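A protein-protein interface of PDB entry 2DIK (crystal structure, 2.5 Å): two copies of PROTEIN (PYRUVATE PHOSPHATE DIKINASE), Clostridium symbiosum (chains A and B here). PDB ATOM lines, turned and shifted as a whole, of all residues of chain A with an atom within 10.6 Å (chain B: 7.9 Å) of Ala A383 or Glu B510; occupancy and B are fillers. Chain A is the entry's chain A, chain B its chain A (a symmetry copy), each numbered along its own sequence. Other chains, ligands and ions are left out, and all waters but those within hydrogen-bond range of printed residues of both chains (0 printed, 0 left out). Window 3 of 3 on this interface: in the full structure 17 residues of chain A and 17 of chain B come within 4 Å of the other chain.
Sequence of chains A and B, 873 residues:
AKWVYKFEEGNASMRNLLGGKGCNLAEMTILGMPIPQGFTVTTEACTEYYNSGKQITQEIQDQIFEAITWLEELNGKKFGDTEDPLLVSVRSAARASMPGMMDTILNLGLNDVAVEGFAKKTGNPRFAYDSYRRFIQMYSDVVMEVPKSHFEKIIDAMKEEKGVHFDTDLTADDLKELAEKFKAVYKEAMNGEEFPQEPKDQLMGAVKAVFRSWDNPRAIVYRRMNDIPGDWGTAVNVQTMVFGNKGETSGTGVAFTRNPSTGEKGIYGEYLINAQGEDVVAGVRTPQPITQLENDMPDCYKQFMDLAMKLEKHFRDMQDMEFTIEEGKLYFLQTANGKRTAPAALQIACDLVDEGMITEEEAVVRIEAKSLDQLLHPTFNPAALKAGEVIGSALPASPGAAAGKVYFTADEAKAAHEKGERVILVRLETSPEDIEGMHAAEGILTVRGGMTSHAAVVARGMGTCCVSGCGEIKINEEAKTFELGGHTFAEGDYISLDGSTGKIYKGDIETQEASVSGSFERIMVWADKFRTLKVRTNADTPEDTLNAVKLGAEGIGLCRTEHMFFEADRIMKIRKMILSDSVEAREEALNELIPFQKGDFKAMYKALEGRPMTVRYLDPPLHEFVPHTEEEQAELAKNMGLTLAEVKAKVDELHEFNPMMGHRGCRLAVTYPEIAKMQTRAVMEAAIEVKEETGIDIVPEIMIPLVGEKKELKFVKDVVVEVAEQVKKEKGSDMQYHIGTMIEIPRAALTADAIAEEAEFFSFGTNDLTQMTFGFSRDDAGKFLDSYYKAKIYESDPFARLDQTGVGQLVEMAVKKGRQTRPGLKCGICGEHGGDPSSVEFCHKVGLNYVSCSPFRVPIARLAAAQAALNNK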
ATOM      1  N   THR A 379      30.972 -31.992  19.169  1.00  0.00           N
ATOM      2  CA  THR A 379      30.663 -32.298  20.531  1.00  0.00           C
ATOM      3  C   THR A 379      29.155 -32.461  20.738  1.00  0.00           C
ATOM      4  O   THR A 379      28.369 -32.687  19.810  1.00  0.00           O
ATOM      5  CB  THR A 379      31.257 -31.277  21.468  1.00  0.00           C
ATOM      6  OG1 THR A 379      30.329 -30.243  21.579  1.00  0.00           O
ATOM      7  CG2 THR A 379      32.498 -30.743  20.783  1.00  0.00           C
ATOM      8  N   PHE A 380      28.727 -32.426  21.992  1.00  0.00           N
ATOM      9  CA  PHE A 380      27.321 -32.595  22.224  1.00  0.00           C
ATOM     10  C   PHE A 380      26.658 -31.284  22.302  1.00  0.00           C
ATOM     11  O   PHE A 380      27.197 -30.340  22.906  1.00  0.00           O
ATOM     12  CB  PHE A 380      26.995 -33.297  23.525  1.00  0.00           C
ATOM     13  CG  PHE A 380      26.765 -34.744  23.294  1.00  0.00           C
ATOM     14  CD1 PHE A 380      26.339 -35.202  22.051  1.00  0.00           C
ATOM     15  CD2 PHE A 380      27.060 -35.674  24.293  1.00  0.00           C
ATOM     16  CE1 PHE A 380      26.146 -36.571  21.851  1.00  0.00           C
ATOM     17  CE2 PHE A 380      26.865 -37.049  24.114  1.00  0.00           C
ATOM     18  CZ  PHE A 380      26.401 -37.485  22.879  1.00  0.00           C
ATOM     19  N   ASN A 381      25.454 -31.289  21.776  1.00  0.00           N
ATOM     20  CA  ASN A 381      24.702 -30.096  21.860  1.00  0.00           C
ATOM     21  C   ASN A 381      24.118 -29.931  23.244  1.00  0.00           C
ATOM     22  O   ASN A 381      23.331 -30.749  23.675  1.00  0.00           O
ATOM     23  CB  ASN A 381      23.586 -30.119  20.844  1.00  0.00           C
ATOM     24  CG  ASN A 381      22.763 -28.878  21.072  1.00  0.00           C
ATOM     25  OD1 ASN A 381      23.303 -27.875  21.590  1.00  0.00           O
ATOM     26  ND2 ASN A 381      21.439 -29.022  20.876  1.00  0.00           N
ATOM     27  N   PRO A 382      24.423 -28.821  23.888  1.00  0.00           N
ATOM     28  CA  PRO A 382      23.942 -28.569  25.220  1.00  0.00           C
ATOM     29  C   PRO A 382      22.468 -28.857  25.498  1.00  0.00           C
ATOM     30  O   PRO A 382      22.124 -29.732  26.302  1.00  0.00           O
ATOM     31  CB  PRO A 382      24.332 -27.130  25.534  1.00  0.00           C
ATOM     32  CG  PRO A 382      25.500 -26.802  24.615  1.00  0.00           C
ATOM     33  CD  PRO A 382      25.409 -27.781  23.460  1.00  0.00           C
ATOM     34  N   ALA A 383      21.576 -28.121  24.872  1.00  0.00           N
ATOM     35  CA  ALA A 383      20.200 -28.409  25.179  1.00  0.00           C
ATOM     36  C   ALA A 383      19.822 -29.825  24.798  1.00  0.00           C
ATOM     37  O   ALA A 383      18.883 -30.356  25.349  1.00  0.00           O
ATOM     38  CB  ALA A 383      19.235 -27.336  24.684  1.00  0.00           C
ATOM     39  N   ALA A 384      20.628 -30.449  23.931  1.00  0.00           N
ATOM     40  CA  ALA A 384      20.411 -31.851  23.506  1.00  0.00           C
ATOM     41  C   ALA A 384      20.627 -32.789  24.683  1.00  0.00           C
ATOM     42  O   ALA A 384      19.853 -33.713  24.940  1.00  0.00           O
ATOM     43  CB  ALA A 384      21.327 -32.287  22.347  1.00  0.00           C
ATOM     44  N   LEU A 385      21.714 -32.526  25.379  1.00  0.00           N
ATOM     45  CA  LEU A 385      22.051 -33.299  26.515  1.00  0.00           C
ATOM     46  C   LEU A 385      21.218 -32.877  27.677  1.00  0.00           C
ATOM     47  O   LEU A 385      20.677 -33.717  28.393  1.00  0.00           O
ATOM     48  CB  LEU A 385      23.506 -33.058  26.872  1.00  0.00           C
ATOM     49  CG  LEU A 385      24.426 -33.843  25.970  1.00  0.00           C
ATOM     50  CD1 LEU A 385      24.176 -33.513  24.492  1.00  0.00           C
ATOM     51  CD2 LEU A 385      25.850 -33.519  26.370  1.00  0.00           C
ATOM     52  N   LYS A 386      21.167 -31.563  27.844  1.00  0.00           N
ATOM     53  CA  LYS A 386      20.439 -30.948  28.932  1.00  0.00           C
ATOM     54  C   LYS A 386      19.068 -31.575  29.042  1.00  0.00           C
ATOM     55  O   LYS A 386      18.642 -32.030  30.108  1.00  0.00           O
ATOM     56  CB  LYS A 386      20.442 -29.432  28.813  1.00  0.00           C
ATOM     57  CG  LYS A 386      19.577 -28.724  29.841  1.00  0.00           C
ATOM     58  CD  LYS A 386      18.174 -28.496  29.294  1.00  0.00           C
ATOM     59  CE  LYS A 386      18.150 -27.959  27.850  1.00  0.00           C
ATOM     60  NZ  LYS A 386      16.843 -28.029  27.142  1.00  0.00           N
ATOM     61  N   ALA A 387      18.490 -31.739  27.880  1.00  0.00           N
ATOM     62  CA  ALA A 387      17.230 -32.377  27.788  1.00  0.00           C
ATOM     63  C   ALA A 387      17.415 -33.800  27.308  1.00  0.00           C
ATOM     64  O   ALA A 387      16.765 -34.198  26.336  1.00  0.00           O
ATOM     65  CB  ALA A 387      16.312 -31.596  26.862  1.00  0.00           C
ATOM     66  N   GLY A 388      18.289 -34.575  27.984  1.00  0.00           N
ATOM     67  CA  GLY A 388      18.558 -35.982  27.599  1.00  0.00           C
ATOM     68  C   GLY A 388      18.330 -37.044  28.697  1.00  0.00           C
ATOM     69  O   GLY A 388      18.541 -36.778  29.905  1.00  0.00           O
ATOM     70  N   GLU A 389      17.932 -38.263  28.258  1.00  0.00           N
ATOM     71  CA  GLU A 389      17.606 -39.375  29.170  1.00  0.00           C
ATOM     72  C   GLU A 389      18.791 -40.099  29.782  1.00  0.00           C
ATOM     73  O   GLU A 389      19.124 -41.192  29.314  1.00  0.00           O
ATOM     74  CB  GLU A 389      16.762 -40.447  28.456  1.00  0.00           C
ATOM     75  CG  GLU A 389      15.589 -41.033  29.285  1.00  0.00           C
ATOM     76  CD  GLU A 389      15.818 -41.039  30.779  1.00  0.00           C
ATOM     77  OE1 GLU A 389      15.973 -40.004  31.438  1.00  0.00           O
ATOM     78  OE2 GLU A 389      15.827 -42.267  31.288  1.00  0.00           O
ATOM     79  N   LYS A 503      23.282 -42.107  28.090  1.00  0.00           N
ATOM     80  CA  LYS A 503      21.870 -41.926  27.948  1.00  0.00           C
ATOM     81  C   LYS A 503      21.278 -42.574  26.697  1.00  0.00           C
ATOM     82  O   LYS A 503      22.034 -43.011  25.812  1.00  0.00           O
ATOM     83  CB  LYS A 503      21.556 -40.444  28.012  1.00  0.00           C
ATOM     84  CG  LYS A 503      22.656 -39.529  27.509  1.00  0.00           C
ATOM     85  CD  LYS A 503      22.477 -38.182  28.143  1.00  0.00           C
ATOM     86  CE  LYS A 503      23.803 -37.527  28.329  1.00  0.00           C
ATOM     87  NZ  LYS A 503      23.865 -36.759  29.593  1.00  0.00           N
ATOM     88  N   ILE A 509      21.203 -38.171  20.586  1.00  0.00           N
ATOM     89  CA  ILE A 509      21.708 -36.831  20.895  1.00  0.00           C
ATOM     90  C   ILE A 509      22.389 -36.033  19.762  1.00  0.00           C
ATOM     91  O   ILE A 509      23.114 -36.540  18.907  1.00  0.00           O
ATOM     92  CB  ILE A 509      22.486 -36.649  22.202  1.00  0.00           C
ATOM     93  CG1 ILE A 509      21.578 -36.862  23.415  1.00  0.00           C
ATOM     94  CG2 ILE A 509      23.142 -35.247  22.284  1.00  0.00           C
ATOM     95  CD1 ILE A 509      21.843 -35.825  24.521  1.00  0.00           C
ATOM     96  N   GLU A 510      22.146 -34.729  19.785  1.00  0.00           N
ATOM     97  CA  GLU A 510      22.709 -33.856  18.814  1.00  0.00           C
ATOM     98  C   GLU A 510      24.113 -33.421  19.167  1.00  0.00           C
ATOM     99  O   GLU A 510      24.443 -32.876  20.239  1.00  0.00           O
ATOM    100  CB  GLU A 510      21.788 -32.663  18.529  1.00  0.00           C
ATOM    101  CG  GLU A 510      22.171 -31.793  17.313  1.00  0.00           C
ATOM    102  CD  GLU A 510      21.240 -30.596  17.189  1.00  0.00           C
ATOM    103  OE1 GLU A 510      21.493 -29.658  18.084  1.00  0.00           O
ATOM    104  OE2 GLU A 510      20.262 -30.558  16.441  1.00  0.00           O
ATOM    105  N   THR A 511      24.908 -33.707  18.167  1.00  0.00           N
ATOM    106  CA  THR A 511      26.295 -33.384  18.098  1.00  0.00           C
ATOM    107  C   THR A 511      26.401 -32.027  17.426  1.00  0.00           C
ATOM    108  O   THR A 511      25.501 -31.616  16.697  1.00  0.00           O
ATOM    109  CB  THR A 511      27.052 -34.490  17.330  1.00  0.00           C
ATOM    110  OG1 THR A 511      26.478 -34.709  16.056  1.00  0.00           O
ATOM    111  CG2 THR A 511      27.017 -35.792  18.127  1.00  0.00           C
ATOM    112  N   GLN A 512      27.463 -31.295  17.681  1.00  0.00           N
ATOM    113  CA  GLN A 512      27.477 -30.004  17.066  1.00  0.00           C
ATOM    114  C   GLN A 512      28.797 -29.542  16.424  1.00  0.00           C
ATOM    115  O   GLN A 512      28.965 -29.678  15.199  1.00  0.00           O
ATOM    116  CB  GLN A 512      26.766 -28.967  17.939  1.00  0.00           C
ATOM    117  CG  GLN A 512      27.549 -28.643  19.209  1.00  0.00           C
ATOM    118  CD  GLN A 512      26.992 -27.412  19.900  1.00  0.00           C
ATOM    119  OE1 GLN A 512      27.710 -26.539  20.448  1.00  0.00           O
ATOM    120  NE2 GLN A 512      25.668 -27.358  19.915  1.00  0.00           N
ATOM    121  N   PRO B 378      26.571 -15.623  26.384  1.00  0.00           N
ATOM    122  CA  PRO B 378      25.833 -16.707  25.777  1.00  0.00           C
ATOM    123  C   PRO B 378      25.826 -16.504  24.290  1.00  0.00           C
ATOM    124  O   PRO B 378      25.313 -15.487  23.807  1.00  0.00           O
ATOM    125  CB  PRO B 378      24.391 -16.475  26.250  1.00  0.00           C
ATOM    126  CG  PRO B 378      24.412 -15.480  27.426  1.00  0.00           C
ATOM    127  CD  PRO B 378      25.849 -15.021  27.572  1.00  0.00           C
ATOM    128  N   THR B 379      26.389 -17.429  23.551  1.00  0.00           N
ATOM    129  CA  THR B 379      26.327 -17.225  22.137  1.00  0.00           C
ATOM    130  C   THR B 379      25.049 -17.823  21.543  1.00  0.00           C
ATOM    131  O   THR B 379      24.049 -18.083  22.222  1.00  0.00           O
ATOM    132  CB  THR B 379      27.567 -17.745  21.455  1.00  0.00           C
ATOM    133  OG1 THR B 379      27.342 -19.094  21.184  1.00  0.00           O
ATOM    134  CG2 THR B 379      28.688 -17.636  22.469  1.00  0.00           C
ATOM    135  N   PHE B 380      25.031 -17.979  20.227  1.00  0.00           N
ATOM    136  CA  PHE B 380      23.841 -18.519  19.633  1.00  0.00           C
ATOM    137  C   PHE B 380      23.966 -19.976  19.480  1.00  0.00           C
ATOM    138  O   PHE B 380      25.037 -20.481  19.100  1.00  0.00           O
ATOM    139  CB  PHE B 380      23.552 -17.984  18.247  1.00  0.00           C
ATOM    140  CG  PHE B 380      22.580 -16.865  18.310  1.00  0.00           C
ATOM    141  CD1 PHE B 380      21.683 -16.768  19.370  1.00  0.00           C
ATOM    142  CD2 PHE B 380      22.615 -15.845  17.358  1.00  0.00           C
ATOM    143  CE1 PHE B 380      20.789 -15.695  19.418  1.00  0.00           C
ATOM    144  CE2 PHE B 380      21.722 -14.767  17.385  1.00  0.00           C
ATOM    145  CZ  PHE B 380      20.806 -14.707  18.428  1.00  0.00           C
ATOM    146  N   ASN B 381      22.832 -20.609  19.681  1.00  0.00           N
ATOM    147  CA  ASN B 381      22.825 -22.009  19.492  1.00  0.00           C
ATOM    148  C   ASN B 381      22.775 -22.347  18.020  1.00  0.00           C
ATOM    149  O   ASN B 381      21.825 -22.002  17.347  1.00  0.00           O
ATOM    150  CB  ASN B 381      21.630 -22.616  20.186  1.00  0.00           C
ATOM    151  CG  ASN B 381      21.625 -24.083  19.843  1.00  0.00           C
ATOM    152  OD1 ASN B 381      22.705 -24.644  19.550  1.00  0.00           O
ATOM    153  ND2 ASN B 381      20.407 -24.632  19.685  1.00  0.00           N
ATOM    154  N   PRO B 382      23.746 -23.109  17.553  1.00  0.00           N
ATOM    155  CA  PRO B 382      23.812 -23.474  16.163  1.00  0.00           C
ATOM    156  C   PRO B 382      22.518 -23.941  15.500  1.00  0.00           C
ATOM    157  O   PRO B 382      22.000 -23.301  14.577  1.00  0.00           O
ATOM    158  CB  PRO B 382      24.933 -24.501  16.059  1.00  0.00           C
ATOM    159  CG  PRO B 382      25.830 -24.265  17.265  1.00  0.00           C
ATOM    160  CD  PRO B 382      24.972 -23.545  18.289  1.00  0.00           C
ATOM    161  N   ALA B 383      21.986 -25.065  15.928  1.00  0.00           N
ATOM    162  CA  ALA B 383      20.780 -25.482  15.262  1.00  0.00           C
ATOM    163  C   ALA B 383      19.665 -24.473  15.435  1.00  0.00           C
ATOM    164  O   ALA B 383      18.762 -24.445  14.628  1.00  0.00           O
ATOM    165  CB  ALA B 383      20.391 -26.924  15.569  1.00  0.00           C
ATOM    166  N   ALA B 384      19.800 -23.592  16.433  1.00  0.00           N
ATOM    167  CA  ALA B 384      18.813 -22.519  16.691  1.00  0.00           C
ATOM    168  C   ALA B 384      18.823 -21.519  15.545  1.00  0.00           C
ATOM    169  O   ALA B 384      17.787 -21.090  15.036  1.00  0.00           O
ATOM    170  CB  ALA B 384      19.060 -21.766  18.011  1.00  0.00           C
ATOM    171  N   LEU B 385      20.033 -21.156  15.168  1.00  0.00           N
ATOM    172  CA  LEU B 385      20.215 -20.241  14.105  1.00  0.00           C
ATOM    173  C   LEU B 385      20.031 -20.940  12.801  1.00  0.00           C
ATOM    174  O   LEU B 385      19.346 -20.435  11.915  1.00  0.00           O
ATOM    175  CB  LEU B 385      21.631 -19.699  14.147  1.00  0.00           C
ATOM    176  CG  LEU B 385      21.773 -18.624  15.196  1.00  0.00           C
ATOM    177  CD1 LEU B 385      21.355 -19.137  16.582  1.00  0.00           C
ATOM    178  CD2 LEU B 385      23.216 -18.166  15.195  1.00  0.00           C
ATOM    179  N   ALA B 401      25.452 -12.071  19.875  1.00  0.00           N
ATOM    180  CA  ALA B 401      24.153 -12.628  19.613  1.00  0.00           C
ATOM    181  C   ALA B 401      23.140 -11.874  20.435  1.00  0.00           C
ATOM    182  O   ALA B 401      23.161 -11.879  21.656  1.00  0.00           O
ATOM    183  CB  ALA B 401      24.117 -14.078  20.020  1.00  0.00           C
ATOM    184  N   ALA B 403      19.131 -10.975  21.407  1.00  0.00           N
ATOM    185  CA  ALA B 403      17.826 -11.514  21.187  1.00  0.00           C
ATOM    186  C   ALA B 403      16.914 -10.949  22.225  1.00  0.00           C
ATOM    187  O   ALA B 403      17.306 -10.931  23.371  1.00  0.00           O
ATOM    188  CB  ALA B 403      17.887 -13.006  21.166  1.00  0.00           C
ATOM    189  N   ARG B 422      16.304  -8.580  27.741  1.00  0.00           N
ATOM    190  CA  ARG B 422      16.133  -8.980  26.362  1.00  0.00           C
ATOM    191  C   ARG B 422      15.347  -7.938  25.585  1.00  0.00           C
ATOM    192  O   ARG B 422      14.147  -8.072  25.352  1.00  0.00           O
ATOM    193  CB  ARG B 422      15.638 -10.397  26.215  1.00  0.00           C
ATOM    194  CG  ARG B 422      16.748 -11.382  26.540  1.00  0.00           C
ATOM    195  CD  ARG B 422      16.317 -12.843  26.355  1.00  0.00           C
ATOM    196  NE  ARG B 422      15.694 -13.161  25.047  1.00  0.00           N
ATOM    197  CZ  ARG B 422      16.182 -14.011  24.101  1.00  0.00           C
ATOM    198  NH1 ARG B 422      17.333 -14.698  24.265  1.00  0.00           N
ATOM    199  NH2 ARG B 422      15.464 -14.194  22.974  1.00  0.00           N
ATOM    200  N   ILE B 495      15.746 -11.005  16.752  1.00  0.00           N
ATOM    201  CA  ILE B 495      16.968 -11.613  17.154  1.00  0.00           C
ATOM    202  C   ILE B 495      18.065 -11.469  16.145  1.00  0.00           C
ATOM    203  O   ILE B 495      17.874 -11.653  14.956  1.00  0.00           O
ATOM    204  CB  ILE B 495      16.722 -13.061  17.401  1.00  0.00           C
ATOM    205  CG1 ILE B 495      15.619 -13.223  18.468  1.00  0.00           C
ATOM    206  CG2 ILE B 495      18.063 -13.620  17.856  1.00  0.00           C
ATOM    207  CD1 ILE B 495      14.459 -14.200  18.123  1.00  0.00           C
ATOM    208  N   ILE B 509      15.574 -16.866  19.271  1.00  0.00           N
ATOM    209  CA  ILE B 509      16.740 -17.751  19.193  1.00  0.00           C
ATOM    210  C   ILE B 509      17.413 -18.180  20.515  1.00  0.00           C
ATOM    211  O   ILE B 509      17.544 -17.439  21.489  1.00  0.00           O
ATOM    212  CB  ILE B 509      17.807 -17.429  18.143  1.00  0.00           C
ATOM    213  CG1 ILE B 509      17.257 -17.614  16.727  1.00  0.00           C
ATOM    214  CG2 ILE B 509      19.071 -18.307  18.328  1.00  0.00           C
ATOM    215  CD1 ILE B 509      18.275 -18.301  15.800  1.00  0.00           C
ATOM    216  N   GLU B 510      17.868 -19.425  20.522  1.00  0.00           N
ATOM    217  CA  GLU B 510      18.523 -19.966  21.662  1.00  0.00           C
ATOM    218  C   GLU B 510      19.994 -19.617  21.709  1.00  0.00           C
ATOM    219  O   GLU B 510      20.811 -19.849  20.797  1.00  0.00           O
ATOM    220  CB  GLU B 510      18.283 -21.476  21.785  1.00  0.00           C
ATOM    221  CG  GLU B 510      18.725 -22.121  23.116  1.00  0.00           C
ATOM    222  CD  GLU B 510      18.520 -23.628  23.083  1.00  0.00           C
ATOM    223  OE1 GLU B 510      19.424 -24.250  22.348  1.00  0.00           O
ATOM    224  OE2 GLU B 510      17.538 -24.201  23.557  1.00  0.00           O
ATOM    225  N   THR B 511      20.255 -19.043  22.856  1.00  0.00           N
ATOM    226  CA  THR B 511      21.548 -18.634  23.298  1.00  0.00           C
ATOM    227  C   THR B 511      22.141 -19.801  24.067  1.00  0.00           C
ATOM    228  O   THR B 511      21.415 -20.656  24.569  1.00  0.00           O
ATOM    229  CB  THR B 511      21.428 -17.355  24.154  1.00  0.00           C
ATOM    230  OG1 THR B 511      20.519 -17.540  25.222  1.00  0.00           O
ATOM    231  CG2 THR B 511      20.952 -16.192  23.287  1.00  0.00           C
ATOM    232  N   GLN B 512      23.451 -19.885  24.142  1.00  0.00           N
ATOM    233  CA  GLN B 512      23.951 -21.037  24.828  1.00  0.00           C
ATOM    234  C   GLN B 512      25.112 -20.821  25.815  1.00  0.00           C
ATOM    235  O   GLN B 512      24.871 -20.706  27.031  1.00  0.00           O
ATOM    236  CB  GLN B 512      24.101 -22.226  23.877  1.00  0.00           C
ATOM    237  CG  GLN B 512      25.234 -22.028  22.874  1.00  0.00           C
ATOM    238  CD  GLN B 512      25.563 -23.321  22.151  1.00  0.00           C
ATOM    239  OE1 GLN B 512      26.733 -23.679  21.866  1.00  0.00           O
ATOM    240  NE2 GLN B 512      24.497 -24.027  21.803  1.00  0.00           N
ATOM    241  N   GLU B 513      26.363 -20.806  25.332  1.00  0.00           N
ATOM    242  CA  GLU B 513      27.504 -20.591  26.230  1.00  0.00           C
ATOM    243  C   GLU B 513      28.819 -20.202  25.535  1.00  0.00           C
ATOM    244  O   GLU B 513      29.011 -20.499  24.348  1.00  0.00           O
ATOM    245  CB  GLU B 513      27.709 -21.714  27.272  1.00  0.00           C
ATOM    246  CG  GLU B 513      28.859 -21.415  28.260  1.00  0.00           C
ATOM    247  CD  GLU B 513      29.017 -22.450  29.339  1.00  0.00           C
ATOM    248  OE1 GLU B 513      28.248 -22.550  30.290  1.00  0.00           O
ATOM    249  OE2 GLU B 513      30.024 -23.246  29.136  1.00  0.00           O
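The side-chain amide oxygen (OE1) of Gln B512 sits close to the side-chain amide oxygen (OE1) of Gln A512 (3.3 Å).
Of chain B, only Glu B510 (3.7 Å) comes within 4 Å of Ala A383.
No residue of chain B comes within 4 Å of Ala A384.
No residue of chain A comes within 4 Å of Phe B380.
Of chain A, only Asn A381 comes within 4 Å of Asn B381.
No residue of chain A comes within 4 Å of Ile B509.
No residue of chain A comes within 4 Å of Thr B511.
Printed residues of chain B within 4 Å of Glu A510: Ala B383.
Printed residues of chain A within 4 Å of Gln B512: Gln A512.
Printed residues of chain B within 4 Å of Gln A512: Gln B512.
Of the printed residues of chain A, Ala B383 touches Glu A510 (3.7 Å).
Thr A511 touches none of the printed residues of chain B.
Pro B382 touches none of the printed residues of chain A.
The nearest residue of chain A that does not touch Glu B510 is Lys A386 (5.3 Å).
The nearest printed residue of chain B that does not touch Glu A510 is Asn B381 (5.4 Å).
Asn A381 touches its own counterpart, Asn B381.
Ala A383 touches Glu B510, and with the chains exchanged Glu A510 touches Ala B383.
Gln B512 touches its own counterpart, Gln A512.
Of the 4 pairs that touch across the chains among the printed residues, 4 have their exchanged pair printed and touching as well.
Asn B381 touches Asn A381 (OD1 to OD1, 3.9 Å).
OE2 of Glu B510 touches CB of Ala A383, 3.7 Å away.
OE2 of Glu A510 touches CB of Ala B383 (3.7 Å).
ND2 of Asn A381 lies close to N of Ala A384 (3.5 Å).
The side-chain amide oxygen of Asn A381 is in hydrogen-bond range of the side-chain amide nitrogen of Gln A512, at 2.9 Å.
O of Thr B379 sits at hydrogen-bond distance from N of Gln B512 (2.7 Å).
ND2 of Asn B381 sits close to N of Ala B384 (3.5 Å).
The backbone NH of Asn B381 sits at hydrogen-bond distance from the backbone carbonyl oxygen of Glu B510 (2.4 Å).
NE2 of Gln B512 lies within hydrogen-bond range of OD1 of Asn B381 (2.9 Å).
Of the 17 printed residues of chain B, 4 touch a printed residue of chain A.
Printed residues of chain B that touch a printed residue of chain A: Asn B381, Ala B383, Glu B510 and Gln B512.
Among the printed residues, 4 pairs touch across the chains.
Among the printed residues, no Asp or Glu carboxylate lies within 4 Å of a Lys or Arg side-chain nitrogen of the other chain.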
